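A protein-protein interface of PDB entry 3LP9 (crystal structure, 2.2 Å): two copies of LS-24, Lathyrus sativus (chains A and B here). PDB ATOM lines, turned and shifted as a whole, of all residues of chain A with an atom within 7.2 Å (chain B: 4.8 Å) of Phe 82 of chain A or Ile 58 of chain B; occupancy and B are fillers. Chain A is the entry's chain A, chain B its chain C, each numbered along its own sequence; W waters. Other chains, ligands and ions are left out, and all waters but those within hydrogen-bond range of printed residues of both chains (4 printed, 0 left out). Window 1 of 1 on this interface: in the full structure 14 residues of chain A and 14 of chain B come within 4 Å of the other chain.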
ATOM      1  N   THR A  57      15.437 -31.301  13.495  1.00  0.00           N
ATOM      2  CA  THR A  57      15.468 -29.843  13.592  1.00  0.00           C
ATOM      3  C   THR A  57      14.894 -29.476  14.962  1.00  0.00           C
ATOM      4  O   THR A  57      14.420 -30.376  15.652  1.00  0.00           O
ATOM      5  CB  THR A  57      14.645 -29.180  12.460  1.00  0.00           C
ATOM      6  OG1 THR A  57      13.260 -29.436  12.706  1.00  0.00           O
ATOM      7  CG2 THR A  57      15.051 -29.709  11.109  1.00  0.00           C
ATOM      8  N   ILE A  58      14.986 -28.201  15.378  1.00  0.00           N
ATOM      9  CA  ILE A  58      14.391 -27.741  16.628  1.00  0.00           C
ATOM     10  C   ILE A  58      12.879 -28.060  16.763  1.00  0.00           C
ATOM     11  O   ILE A  58      12.423 -28.447  17.857  1.00  0.00           O
ATOM     12  CB  ILE A  58      14.656 -26.236  16.900  1.00  0.00           C
ATOM     13  CG1 ILE A  58      14.109 -25.341  15.763  1.00  0.00           C
ATOM     14  CG2 ILE A  58      16.173 -25.970  17.068  1.00  0.00           C
ATOM     15  CD1 ILE A  58      14.270 -23.894  16.033  1.00  0.00           C
ATOM     16  N   PHE A  59      12.134 -27.941  15.656  1.00  0.00           N
ATOM     17  CA  PHE A  59      10.667 -28.236  15.558  1.00  0.00           C
ATOM     18  C   PHE A  59      10.358 -29.668  15.795  1.00  0.00           C
ATOM     19  O   PHE A  59       9.317 -29.978  16.360  1.00  0.00           O
ATOM     20  CB  PHE A  59      10.144 -27.881  14.206  1.00  0.00           C
ATOM     21  CG  PHE A  59      10.441 -26.446  13.810  1.00  0.00           C
ATOM     22  CD1 PHE A  59       9.878 -25.394  14.524  1.00  0.00           C
ATOM     23  CD2 PHE A  59      11.342 -26.166  12.746  1.00  0.00           C
ATOM     24  CE1 PHE A  59      10.148 -24.103  14.220  1.00  0.00           C
ATOM     25  CE2 PHE A  59      11.618 -24.813  12.350  1.00  0.00           C
ATOM     26  CZ  PHE A  59      11.009 -23.763  13.092  1.00  0.00           C
ATOM     27  N   ASP A  65       5.247 -23.945  18.399  1.00  0.00           N
ATOM     28  CA  ASP A  65       4.415 -23.149  19.338  1.00  0.00           C
ATOM     29  C   ASP A  65       3.586 -22.023  18.762  1.00  0.00           C
ATOM     30  O   ASP A  65       2.784 -21.473  19.446  1.00  0.00           O
ATOM     31  CB  ASP A  65       5.263 -22.653  20.481  1.00  0.00           C
ATOM     32  CG  ASP A  65       6.340 -21.698  20.028  1.00  0.00           C
ATOM     33  OD1 ASP A  65       6.114 -20.938  19.003  1.00  0.00           O
ATOM     34  OD2 ASP A  65       7.357 -21.633  20.761  1.00  0.00           O
ATOM     35  N   CYS A  66       3.741 -21.707  17.488  1.00  0.00           N
ATOM     36  CA  CYS A  66       2.894 -20.763  16.804  1.00  0.00           C
ATOM     37  C   CYS A  66       3.003 -21.134  15.305  1.00  0.00           C
ATOM     38  O   CYS A  66       3.970 -21.810  14.890  1.00  0.00           O
ATOM     39  CB  CYS A  66       3.329 -19.319  17.064  1.00  0.00           C
ATOM     40  SG  CYS A  66       2.255 -18.034  16.269  1.00  0.00           S
ATOM     41  N   ILE A  77       5.900 -21.796  10.746  1.00  0.00           N
ATOM     42  CA  ILE A  77       5.891 -22.418  12.075  1.00  0.00           C
ATOM     43  C   ILE A  77       6.929 -21.713  12.913  1.00  0.00           C
ATOM     44  O   ILE A  77       7.862 -21.106  12.385  1.00  0.00           O
ATOM     45  CB  ILE A  77       6.179 -23.965  12.011  1.00  0.00           C
ATOM     46  CG1 ILE A  77       7.524 -24.287  11.350  1.00  0.00           C
ATOM     47  CG2 ILE A  77       5.041 -24.658  11.274  1.00  0.00           C
ATOM     48  CD1 ILE A  77       7.849 -25.744  11.250  1.00  0.00           C
ATOM     49  N   PHE A  78       6.745 -21.729  14.222  1.00  0.00           N
ATOM     50  CA  PHE A  78       7.658 -21.003  15.147  1.00  0.00           C
ATOM     51  C   PHE A  78       7.935 -21.954  16.318  1.00  0.00           C
ATOM     52  O   PHE A  78       7.110 -22.822  16.622  1.00  0.00           O
ATOM     53  CB  PHE A  78       6.999 -19.713  15.646  1.00  0.00           C
ATOM     54  CG  PHE A  78       6.667 -18.704  14.569  1.00  0.00           C
ATOM     55  CD1 PHE A  78       7.417 -17.590  14.421  1.00  0.00           C
ATOM     56  CD2 PHE A  78       5.566 -18.881  13.730  1.00  0.00           C
ATOM     57  CE1 PHE A  78       7.133 -16.616  13.407  1.00  0.00           C
ATOM     58  CE2 PHE A  78       5.205 -17.902  12.727  1.00  0.00           C
ATOM     59  CZ  PHE A  78       6.045 -16.769  12.562  1.00  0.00           C
ATOM     60  N   TYR A  79       9.102 -21.781  16.953  1.00  0.00           N
ATOM     61  CA  TYR A  79       9.416 -22.403  18.208  1.00  0.00           C
ATOM     62  C   TYR A  79      10.343 -21.426  18.874  1.00  0.00           C
ATOM     63  O   TYR A  79      11.507 -21.236  18.442  1.00  0.00           O
ATOM     64  CB  TYR A  79      10.129 -23.765  18.065  1.00  0.00           C
ATOM     65  CG  TYR A  79      10.610 -24.246  19.420  1.00  0.00           C
ATOM     66  CD1 TYR A  79       9.694 -24.691  20.379  1.00  0.00           C
ATOM     67  CD2 TYR A  79      11.979 -24.158  19.786  1.00  0.00           C
ATOM     68  CE1 TYR A  79      10.129 -25.069  21.675  1.00  0.00           C
ATOM     69  CE2 TYR A  79      12.413 -24.537  21.089  1.00  0.00           C
ATOM     70  CZ  TYR A  79      11.480 -24.966  22.012  1.00  0.00           C
ATOM     71  OH  TYR A  79      11.875 -25.376  23.258  1.00  0.00           O
ATOM     72  N   GLU A  80       9.836 -20.812  19.949  1.00  0.00           N
ATOM     73  CA  GLU A  80      10.592 -19.781  20.657  1.00  0.00           C
ATOM     74  C   GLU A  80      11.000 -18.671  19.675  1.00  0.00           C
ATOM     75  O   GLU A  80      10.115 -18.067  19.015  1.00  0.00           O
ATOM     76  CB  GLU A  80      11.740 -20.414  21.500  1.00  0.00           C
ATOM     77  CG  GLU A  80      11.216 -21.347  22.576  1.00  0.00           C
ATOM     78  CD  GLU A  80      12.295 -21.855  23.486  1.00  0.00           C
ATOM     79  OE1 GLU A  80      13.496 -21.734  23.147  1.00  0.00           O
ATOM     80  OE2 GLU A  80      11.964 -22.370  24.553  1.00  0.00           O
ATOM     81  N   ASN A  81      12.306 -18.401  19.541  1.00  0.00           N
ATOM     82  CA  ASN A  81      12.769 -17.285  18.662  1.00  0.00           C
ATOM     83  C   ASN A  81      13.059 -17.590  17.177  1.00  0.00           C
ATOM     84  O   ASN A  81      13.483 -16.724  16.412  1.00  0.00           O
ATOM     85  CB  ASN A  81      13.990 -16.558  19.326  1.00  0.00           C
ATOM     86  CG  ASN A  81      15.111 -17.474  19.633  1.00  0.00           C
ATOM     87  OD1 ASN A  81      14.882 -18.612  20.099  1.00  0.00           O
ATOM     88  ND2 ASN A  81      16.371 -17.022  19.356  1.00  0.00           N
ATOM     89  N   PHE A  82      12.855 -18.857  16.818  1.00  0.00           N
ATOM     90  CA  PHE A  82      13.111 -19.383  15.457  1.00  0.00           C
ATOM     91  C   PHE A  82      11.799 -19.622  14.749  1.00  0.00           C
ATOM     92  O   PHE A  82      10.739 -19.762  15.381  1.00  0.00           O
ATOM     93  CB  PHE A  82      13.964 -20.661  15.537  1.00  0.00           C
ATOM     94  CG  PHE A  82      15.332 -20.433  16.136  1.00  0.00           C
ATOM     95  CD1 PHE A  82      16.442 -20.114  15.323  1.00  0.00           C
ATOM     96  CD2 PHE A  82      15.540 -20.525  17.538  1.00  0.00           C
ATOM     97  CE1 PHE A  82      17.729 -19.879  15.879  1.00  0.00           C
ATOM     98  CE2 PHE A  82      16.779 -20.279  18.076  1.00  0.00           C
ATOM     99  CZ  PHE A  82      17.869 -19.965  17.238  1.00  0.00           C
ATOM    100  N   CYS A  83      11.838 -19.552  13.424  1.00  0.00           N
ATOM    101  CA  CYS A  83      10.679 -19.844  12.602  1.00  0.00           C
ATOM    102  C   CYS A  83      11.087 -20.482  11.269  1.00  0.00           C
ATOM    103  O   CYS A  83      12.256 -20.424  10.831  1.00  0.00           O
ATOM    104  CB  CYS A  83       9.848 -18.591  12.353  1.00  0.00           C
ATOM    105  SG  CYS A  83      10.537 -17.525  11.198  1.00  0.00           S
ATOM    106  N   ALA A  84      10.129 -21.108  10.619  1.00  0.00           N
ATOM    107  CA  ALA A  84      10.415 -21.790   9.325  1.00  0.00           C
ATOM    108  C   ALA A  84       9.184 -21.712   8.415  1.00  0.00           C
ATOM    109  O   ALA A  84       8.047 -21.700   8.901  1.00  0.00           O
ATOM    110  CB  ALA A  84      10.891 -23.235   9.548  1.00  0.00           C
ATOM    111  N   GLY A 100      14.515 -21.280   6.249  1.00  0.00           N
ATOM    112  CA  GLY A 100      14.971 -21.475   7.626  1.00  0.00           C
ATOM    113  C   GLY A 100      15.391 -22.921   7.998  1.00  0.00           C
ATOM    114  O   GLY A 100      15.707 -23.710   7.103  1.00  0.00           O
ATOM    115  N   PRO A 101      15.385 -23.264   9.298  1.00  0.00           N
ATOM    116  CA  PRO A 101      15.029 -22.387  10.442  1.00  0.00           C
ATOM    117  C   PRO A 101      15.845 -21.084  10.562  1.00  0.00           C
ATOM    118  O   PRO A 101      17.054 -21.068  10.453  1.00  0.00           O
ATOM    119  CB  PRO A 101      15.186 -23.303  11.674  1.00  0.00           C
ATOM    120  CG  PRO A 101      15.088 -24.764  11.101  1.00  0.00           C
ATOM    121  CD  PRO A 101      15.723 -24.638   9.743  1.00  0.00           C
ATOM    122  N   LYS A 102      15.118 -19.975  10.734  1.00  0.00           N
ATOM    123  CA  LYS A 102      15.718 -18.654  10.949  1.00  0.00           C
ATOM    124  C   LYS A 102      15.073 -17.910  12.123  1.00  0.00           C
ATOM    125  O   LYS A 102      13.917 -18.053  12.410  1.00  0.00           O
ATOM    126  CB  LYS A 102      15.592 -17.785   9.677  1.00  0.00           C
ATOM    127  CG  LYS A 102      16.712 -17.951   8.645  1.00  0.00           C
ATOM    128  CD  LYS A 102      16.637 -16.757   7.677  1.00  0.00           C
ATOM    129  CE  LYS A 102      17.575 -16.934   6.497  1.00  0.00           C
ATOM    130  NZ  LYS A 102      16.760 -17.640   5.445  1.00  0.00           N
ATOM    131  N   LYS A 103      15.856 -17.062  12.779  1.00  0.00           N
ATOM    132  CA  LYS A 103      15.390 -16.264  13.890  1.00  0.00           C
ATOM    133  C   LYS A 103      14.212 -15.406  13.386  1.00  0.00           C
ATOM    134  O   LYS A 103      14.278 -14.883  12.301  1.00  0.00           O
ATOM    135  CB  LYS A 103      16.547 -15.383  14.362  1.00  0.00           C
ATOM    136  CG  LYS A 103      17.385 -15.982  15.517  1.00  0.00           C
ATOM    137  CD  LYS A 103      18.746 -15.384  15.519  1.00  0.00           C
ATOM    138  CE  LYS A 103      19.494 -15.763  16.743  1.00  0.00           C
ATOM    139  NZ  LYS A 103      20.840 -15.083  16.813  1.00  0.00           N
ATOM    140  N   ILE A 104      13.170 -15.258  14.197  1.00  0.00           N
ATOM    141  CA  ILE A 104      12.028 -14.449  13.856  1.00  0.00           C
ATOM    142  C   ILE A 104      12.440 -13.055  13.403  1.00  0.00           C
ATOM    143  O   ILE A 104      12.027 -12.616  12.338  1.00  0.00           O
ATOM    144  CB  ILE A 104      11.033 -14.350  15.047  1.00  0.00           C
ATOM    145  CG1 ILE A 104      10.402 -15.714  15.362  1.00  0.00           C
ATOM    146  CG2 ILE A 104      10.012 -13.270  14.841  1.00  0.00           C
ATOM    147  CD1 ILE A 104       9.807 -15.761  16.708  1.00  0.00           C
ATOM    148  N   ALA A 105      13.264 -12.374  14.218  1.00  0.00           N
ATOM    149  CA  ALA A 105      13.769 -11.013  13.938  1.00  0.00           C
ATOM    150  C   ALA A 105      14.485 -10.905  12.569  1.00  0.00           C
ATOM    151  O   ALA A 105      14.578  -9.853  11.969  1.00  0.00           O
ATOM    152  CB  ALA A 105      14.691 -10.633  15.031  1.00  0.00           C
ATOM    153  N   GLU A 117      10.017 -10.621  18.999  1.00  0.00           N
ATOM    154  CA  GLU A 117      11.347 -11.097  18.623  1.00  0.00           C
ATOM    155  C   GLU A 117      11.679 -12.458  19.206  1.00  0.00           C
ATOM    156  O   GLU A 117      12.191 -13.335  18.506  1.00  0.00           O
ATOM    157  CB  GLU A 117      12.422 -10.063  18.956  1.00  0.00           C
ATOM    158  CG  GLU A 117      13.832 -10.486  18.524  1.00  0.00           C
ATOM    159  CD  GLU A 117      14.875  -9.434  18.833  1.00  0.00           C
ATOM    160  OE1 GLU A 117      14.499  -8.250  19.117  1.00  0.00           O
ATOM    161  OE2 GLU A 117      16.070  -9.776  18.790  1.00  0.00           O
ATOM    162  N   SER A 118      11.390 -12.605  20.495  1.00  0.00           N
ATOM    163  CA  SER A 118      11.705 -13.799  21.311  1.00  0.00           C
ATOM    164  C   SER A 118      10.622 -14.894  21.190  1.00  0.00           C
ATOM    165  O   SER A 118      10.769 -15.994  21.750  1.00  0.00           O
ATOM    166  CB  SER A 118      11.838 -13.396  22.797  1.00  0.00           C
ATOM    167  OG  SER A 118      10.548 -13.046  23.310  1.00  0.00           O
ATOM    168  N   GLY A 119       9.558 -14.574  20.456  1.00  0.00           N
ATOM    169  CA  GLY A 119       8.460 -15.518  20.284  1.00  0.00           C
ATOM    170  C   GLY A 119       7.043 -14.986  20.128  1.00  0.00           C
ATOM    171  O   GLY A 119       6.701 -13.858  20.528  1.00  0.00           O
ATOM    172  N   GLN B  56      19.340 -27.117   6.109  1.00  0.00           N
ATOM    173  CA  GLN B  56      18.076 -26.585   6.612  1.00  0.00           C
ATOM    174  C   GLN B  56      17.942 -26.800   8.106  1.00  0.00           C
ATOM    175  O   GLN B  56      17.070 -27.486   8.574  1.00  0.00           O
ATOM    176  CB  GLN B  56      16.941 -27.241   5.868  1.00  0.00           C
ATOM    177  CG  GLN B  56      16.950 -26.792   4.390  1.00  0.00           C
ATOM    178  CD  GLN B  56      15.768 -27.254   3.573  1.00  0.00           C
ATOM    179  OE1 GLN B  56      15.600 -28.459   3.303  1.00  0.00           O
ATOM    180  NE2 GLN B  56      14.977 -26.320   3.140  1.00  0.00           N
ATOM    181  N   THR B  57      18.874 -26.207   8.849  1.00  0.00           N
ATOM    182  CA  THR B  57      18.905 -26.234  10.316  1.00  0.00           C
ATOM    183  C   THR B  57      19.486 -24.896  10.749  1.00  0.00           C
ATOM    184  O   THR B  57      19.910 -24.084   9.875  1.00  0.00           O
ATOM    185  CB  THR B  57      19.834 -27.364  10.883  1.00  0.00           C
ATOM    186  OG1 THR B  57      21.211 -27.052  10.606  1.00  0.00           O
ATOM    187  CG2 THR B  57      19.483 -28.687  10.305  1.00  0.00           C
ATOM    188  N   ILE B  58      19.485 -24.638  12.061  1.00  0.00           N
ATOM    189  CA  ILE B  58      19.989 -23.379  12.646  1.00  0.00           C
ATOM    190  C   ILE B  58      21.493 -23.231  12.306  1.00  0.00           C
ATOM    191  O   ILE B  58      22.029 -22.124  12.145  1.00  0.00           O
ATOM    192  CB  ILE B  58      19.735 -23.335  14.202  1.00  0.00           C
ATOM    193  CG1 ILE B  58      20.253 -24.646  14.821  1.00  0.00           C
ATOM    194  CG2 ILE B  58      18.292 -23.129  14.439  1.00  0.00           C
ATOM    195  CD1 ILE B  58      20.080 -24.880  16.347  1.00  0.00           C
ATOM    196  N   PHE B  59      22.170 -24.384  12.181  1.00  0.00           N
ATOM    197  CA  PHE B  59      23.570 -24.420  11.758  1.00  0.00           C
ATOM    198  C   PHE B  59      23.802 -24.053  10.287  1.00  0.00           C
ATOM    199  O   PHE B  59      24.826 -23.448   9.951  1.00  0.00           O
ATOM    200  CB  PHE B  59      24.165 -25.777  12.052  1.00  0.00           C
ATOM    201  CG  PHE B  59      23.901 -26.234  13.440  1.00  0.00           C
ATOM    202  CD1 PHE B  59      24.513 -25.601  14.526  1.00  0.00           C
ATOM    203  CD2 PHE B  59      22.994 -27.301  13.682  1.00  0.00           C
ATOM    204  CE1 PHE B  59      24.273 -26.020  15.831  1.00  0.00           C
ATOM    205  CE2 PHE B  59      22.727 -27.729  15.033  1.00  0.00           C
ATOM    206  CZ  PHE B  59      23.379 -27.060  16.089  1.00  0.00           C
ATOM    207  N   GLY B  60      22.900 -24.458   9.402  1.00  0.00           N
ATOM    208  CA  GLY B  60      23.057 -24.111   8.019  1.00  0.00           C
ATOM    209  C   GLY B  60      22.842 -22.622   7.893  1.00  0.00           C
ATOM    210  O   GLY B  60      23.570 -21.972   7.200  1.00  0.00           O
ATOM    211  N   SER B  61      21.812 -22.107   8.564  1.00  0.00           N
ATOM    212  CA  SER B  61      21.475 -20.669   8.625  1.00  0.00           C
ATOM    213  C   SER B  61      22.563 -19.762   9.251  1.00  0.00           C
ATOM    214  O   SER B  61      22.954 -18.758   8.678  1.00  0.00           O
ATOM    215  CB  SER B  61      20.150 -20.474   9.340  1.00  0.00           C
ATOM    216  OG  SER B  61      19.043 -20.872   8.538  1.00  0.00           O
ATOM    217  N   TYR B  62      23.076 -20.103  10.405  1.00  0.00           N
ATOM    218  CA  TYR B  62      23.979 -19.191  11.174  1.00  0.00           C
ATOM    219  C   TYR B  62      25.413 -19.606  11.366  1.00  0.00           C
ATOM    220  O   TYR B  62      26.254 -18.781  11.738  1.00  0.00           O
ATOM    221  CB  TYR B  62      23.316 -18.838  12.534  1.00  0.00           C
ATOM    222  CG  TYR B  62      21.991 -18.143  12.347  1.00  0.00           C
ATOM    223  CD1 TYR B  62      21.947 -16.820  11.956  1.00  0.00           C
ATOM    224  CD2 TYR B  62      20.789 -18.828  12.556  1.00  0.00           C
ATOM    225  CE1 TYR B  62      20.738 -16.168  11.758  1.00  0.00           C
ATOM    226  CE2 TYR B  62      19.562 -18.184  12.372  1.00  0.00           C
ATOM    227  CZ  TYR B  62      19.552 -16.880  11.953  1.00  0.00           C
ATOM    228  OH  TYR B  62      18.381 -16.284  11.800  1.00  0.00           O
ATOM    229  N   GLY B  63      25.672 -20.897  11.184  1.00  0.00           N
ATOM    230  CA  GLY B  63      27.001 -21.436  11.342  1.00  0.00           C
ATOM    231  C   GLY B  63      27.130 -22.118  12.671  1.00  0.00           C
ATOM    232  O   GLY B  63      26.147 -22.368  13.355  1.00  0.00           O
ATOM    233  N   TYR B  79      25.471 -23.640  18.521  1.00  0.00           N
ATOM    234  CA  TYR B  79      25.048 -22.340  17.989  1.00  0.00           C
ATOM    235  C   TYR B  79      24.150 -21.744  19.097  1.00  0.00           C
ATOM    236  O   TYR B  79      23.084 -22.267  19.360  1.00  0.00           O
ATOM    237  CB  TYR B  79      24.310 -22.471  16.649  1.00  0.00           C
ATOM    238  CG  TYR B  79      23.833 -21.118  16.259  1.00  0.00           C
ATOM    239  CD1 TYR B  79      24.748 -20.158  15.875  1.00  0.00           C
ATOM    240  CD2 TYR B  79      22.506 -20.725  16.468  1.00  0.00           C
ATOM    241  CE1 TYR B  79      24.371 -18.863  15.642  1.00  0.00           C
ATOM    242  CE2 TYR B  79      22.092 -19.413  16.202  1.00  0.00           C
ATOM    243  CZ  TYR B  79      23.019 -18.499  15.805  1.00  0.00           C
ATOM    244  OH  TYR B  79      22.659 -17.190  15.557  1.00  0.00           O
ATOM    245  N   GLU B  80      24.640 -20.725  19.820  1.00  0.00           N
ATOM    246  CA  GLU B  80      23.884 -20.145  20.941  1.00  0.00           C
ATOM    247  C   GLU B  80      23.475 -21.221  21.918  1.00  0.00           C
ATOM    248  O   GLU B  80      24.336 -21.969  22.348  1.00  0.00           O
ATOM    249  CB  GLU B  80      22.695 -19.297  20.458  1.00  0.00           C
ATOM    250  CG  GLU B  80      23.075 -18.329  19.333  1.00  0.00           C
ATOM    251  CD  GLU B  80      22.131 -17.158  19.185  1.00  0.00           C
ATOM    252  OE1 GLU B  80      20.943 -17.310  19.492  1.00  0.00           O
ATOM    253  OE2 GLU B  80      22.596 -16.080  18.731  1.00  0.00           O
ATOM    254  N   PHE B  82      21.814 -23.991  21.407  1.00  0.00           N
ATOM    255  CA  PHE B  82      21.502 -25.293  20.777  1.00  0.00           C
ATOM    256  C   PHE B  82      22.776 -26.009  20.401  1.00  0.00           C
ATOM    257  O   PHE B  82      23.784 -25.377  20.151  1.00  0.00           O
ATOM    258  CB  PHE B  82      20.576 -25.132  19.543  1.00  0.00           C
ATOM    259  CG  PHE B  82      19.173 -24.712  19.880  1.00  0.00           C
ATOM    260  CD1 PHE B  82      18.183 -25.666  20.100  1.00  0.00           C
ATOM    261  CD2 PHE B  82      18.842 -23.370  20.019  1.00  0.00           C
ATOM    262  CE1 PHE B  82      16.864 -25.270  20.467  1.00  0.00           C
ATOM    263  CE2 PHE B  82      17.550 -22.997  20.389  1.00  0.00           C
ATOM    264  CZ  PHE B  82      16.586 -23.929  20.602  1.00  0.00           C
ATOM    265  N   PRO B 101      18.975 -31.141  16.338  1.00  0.00           N
ATOM    266  CA  PRO B 101      19.406 -29.993  17.143  1.00  0.00           C
ATOM    267  C   PRO B 101      18.681 -29.903  18.455  1.00  0.00           C
ATOM    268  O   PRO B 101      17.462 -30.088  18.530  1.00  0.00           O
ATOM    269  CB  PRO B 101      19.077 -28.787  16.259  1.00  0.00           C
ATOM    270  CG  PRO B 101      19.146 -29.355  14.858  1.00  0.00           C
ATOM    271  CD  PRO B 101      18.504 -30.701  15.014  1.00  0.00           C
HETATM  272  O   HOH W   1      18.944 -18.682  20.244  1.00  0.00           O
HETATM  273  O   HOH W   2      20.070 -14.292  19.619  1.00  0.00           O
HETATM  274  O   HOH W   3      17.252 -26.791  13.431  1.00  0.00           O
HETATM  275  O   HOH W   4      15.782 -23.677   4.244  1.00  0.00           O
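O of Pro 101 of chain A lies within hydrogen-bond range of OG of Ser 61 of chain B. The backbone NH (N) of Lys 103 of chain A is in hydrogen-bond range of the side-chain hydroxyl (OH) of Tyr 62 of chain B (2.8 Å). The side-chain amino group of Lys 103 of chain A lies within hydrogen-bond range of the side-chain hydroxyl of Tyr 79 of chain B (3.1 Å). The side-chain amino group of Lys 103 of chain A is in salt-bridge range of the side-chain carboxylate of Glu 80 of chain B (2.8 Å).
The side-chain hydroxyl of Thr 57 of chain A lies close to the backbone NH of Phe 59 of chain A, 3.5 Å away. The backbone carbonyl oxygen of Lys 102 of chain A is in hydrogen-bond range of the backbone NH of Cys 83 of chain A (2.8 Å). The side-chain hydroxyl (OG1) of Thr 57 of chain B lies close to the backbone NH (N) of Phe 59 of chain B, 3.2 Å away. The side-chain hydroxyl (OG1) of Thr 57 of chain B lies within hydrogen-bond range of the backbone NH (N) of Gly 60 of chain B (3.3 Å). The side-chain carboxylate (OE2) of Glu 80 of chain B is in hydrogen-bond range of the side-chain hydroxyl (OH) of Tyr 79 of chain B (3.4 Å).
Among the printed residues, pairs that only touch across the chains: Pro 101 of chain A with Gln 56 of chain B (3.4 Å), Thr 57 of chain A with Pro 101 of chain B (3.5 Å), Ile 58 of chain A with Phe 82 of chain B (3.5 Å), Phe 82 of chain A with Ile 58 of chain B (3.6 Å), Pro 101 of chain A with Thr 57 of chain B (3.6 Å), Phe 82 of chain A with Phe 82 of chain B (3.7 Å), Lys 102 of chain A with Tyr 62 of chain B (3.7 Å), Lys 102 of chain A with Ser 61 of chain B (3.7 Å), Gly 100 of chain A with Gln 56 of chain B (3.8 Å) and Thr 57 of chain A with Gln 56 of chain B (3.9 Å).
Phe 82 of chain A touches just these residues of chain B: Ile 58 and Phe 82. Of chain A, only Phe 82 comes within 4 Å of Ile 58 of chain B. Of the printed residues of chain A, Pro 101 of chain B touches Thr 57. Of the printed residues of chain B, Pro 101 of chain A touches Gln 56 (3.4 Å), Thr 57 (3.6 Å) and Ser 61 (2.8 Å). Printed residues of chain A within 4 Å of Phe 82 of chain B: Ile 58 (3.5 Å) and Phe 82 (3.7 Å). Ile 77 of chain A touches none of the printed residues of chain B. Gly 60 of chain B touches none of the printed residues of chain A. The nearest residue of chain B that does not touch Phe 82 of chain A is Tyr 62 of chain B (4.3 Å). The nearest printed residue of chain A that does not touch Thr 57 of chain B is Gly 100 of chain A (4.4 Å).
Of the 22 printed residues of chain A, 7 touch a printed residue of chain B. Printed residues of chain B that touch a printed residue of chain A: Gln 56, Thr 57, Ile 58, Ser 61, Tyr 62, Tyr 79, Glu 80, Phe 82 and Pro 101. Hydrophobic or aromatic side chains of chain B that line the printed part of chain A: Ile 58, Tyr 62, Tyr 79, Phe 82 and Pro 101. Among the printed residues, 14 pairs touch across the chains.
Thr 57 of chain A touches Pro 101 of chain B, and with the chains exchanged Pro 101 of chain A touches Thr 57 of chain B. Ile 58 of chain A touches Phe 82 of chain B, and with the chains exchanged Phe 82 of chain A touches Ile 58 of chain B. Phe 82 of chain A touches its own counterpart, Phe 82 of chain B. Positions printed for both chains: 57, 58, 59, 79, 80, 82 and 101.
Water W1 lies within hydrogen-bond range of OE1 of Glu 80 of chain B and ND2 of Asn 81 of chain A. Water W4 bridges the backbone carbonyl oxygen of Gly 100 of chain A (2.9 Å) and the side-chain amide nitrogen of Gln 56 of chain B (3.0 Å). Water W2 bridges the side-chain amino group (NZ) of Lys 103 of chain A (3.0 Å) and the side-chain carboxylate (OE1) of Glu 80 of chain B (3.1 Å). Water W3 bridges the backbone NH of Ile 58 of chain A (3.3 Å) and the backbone NH of Ile 58 of chain B (3.4 Å).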
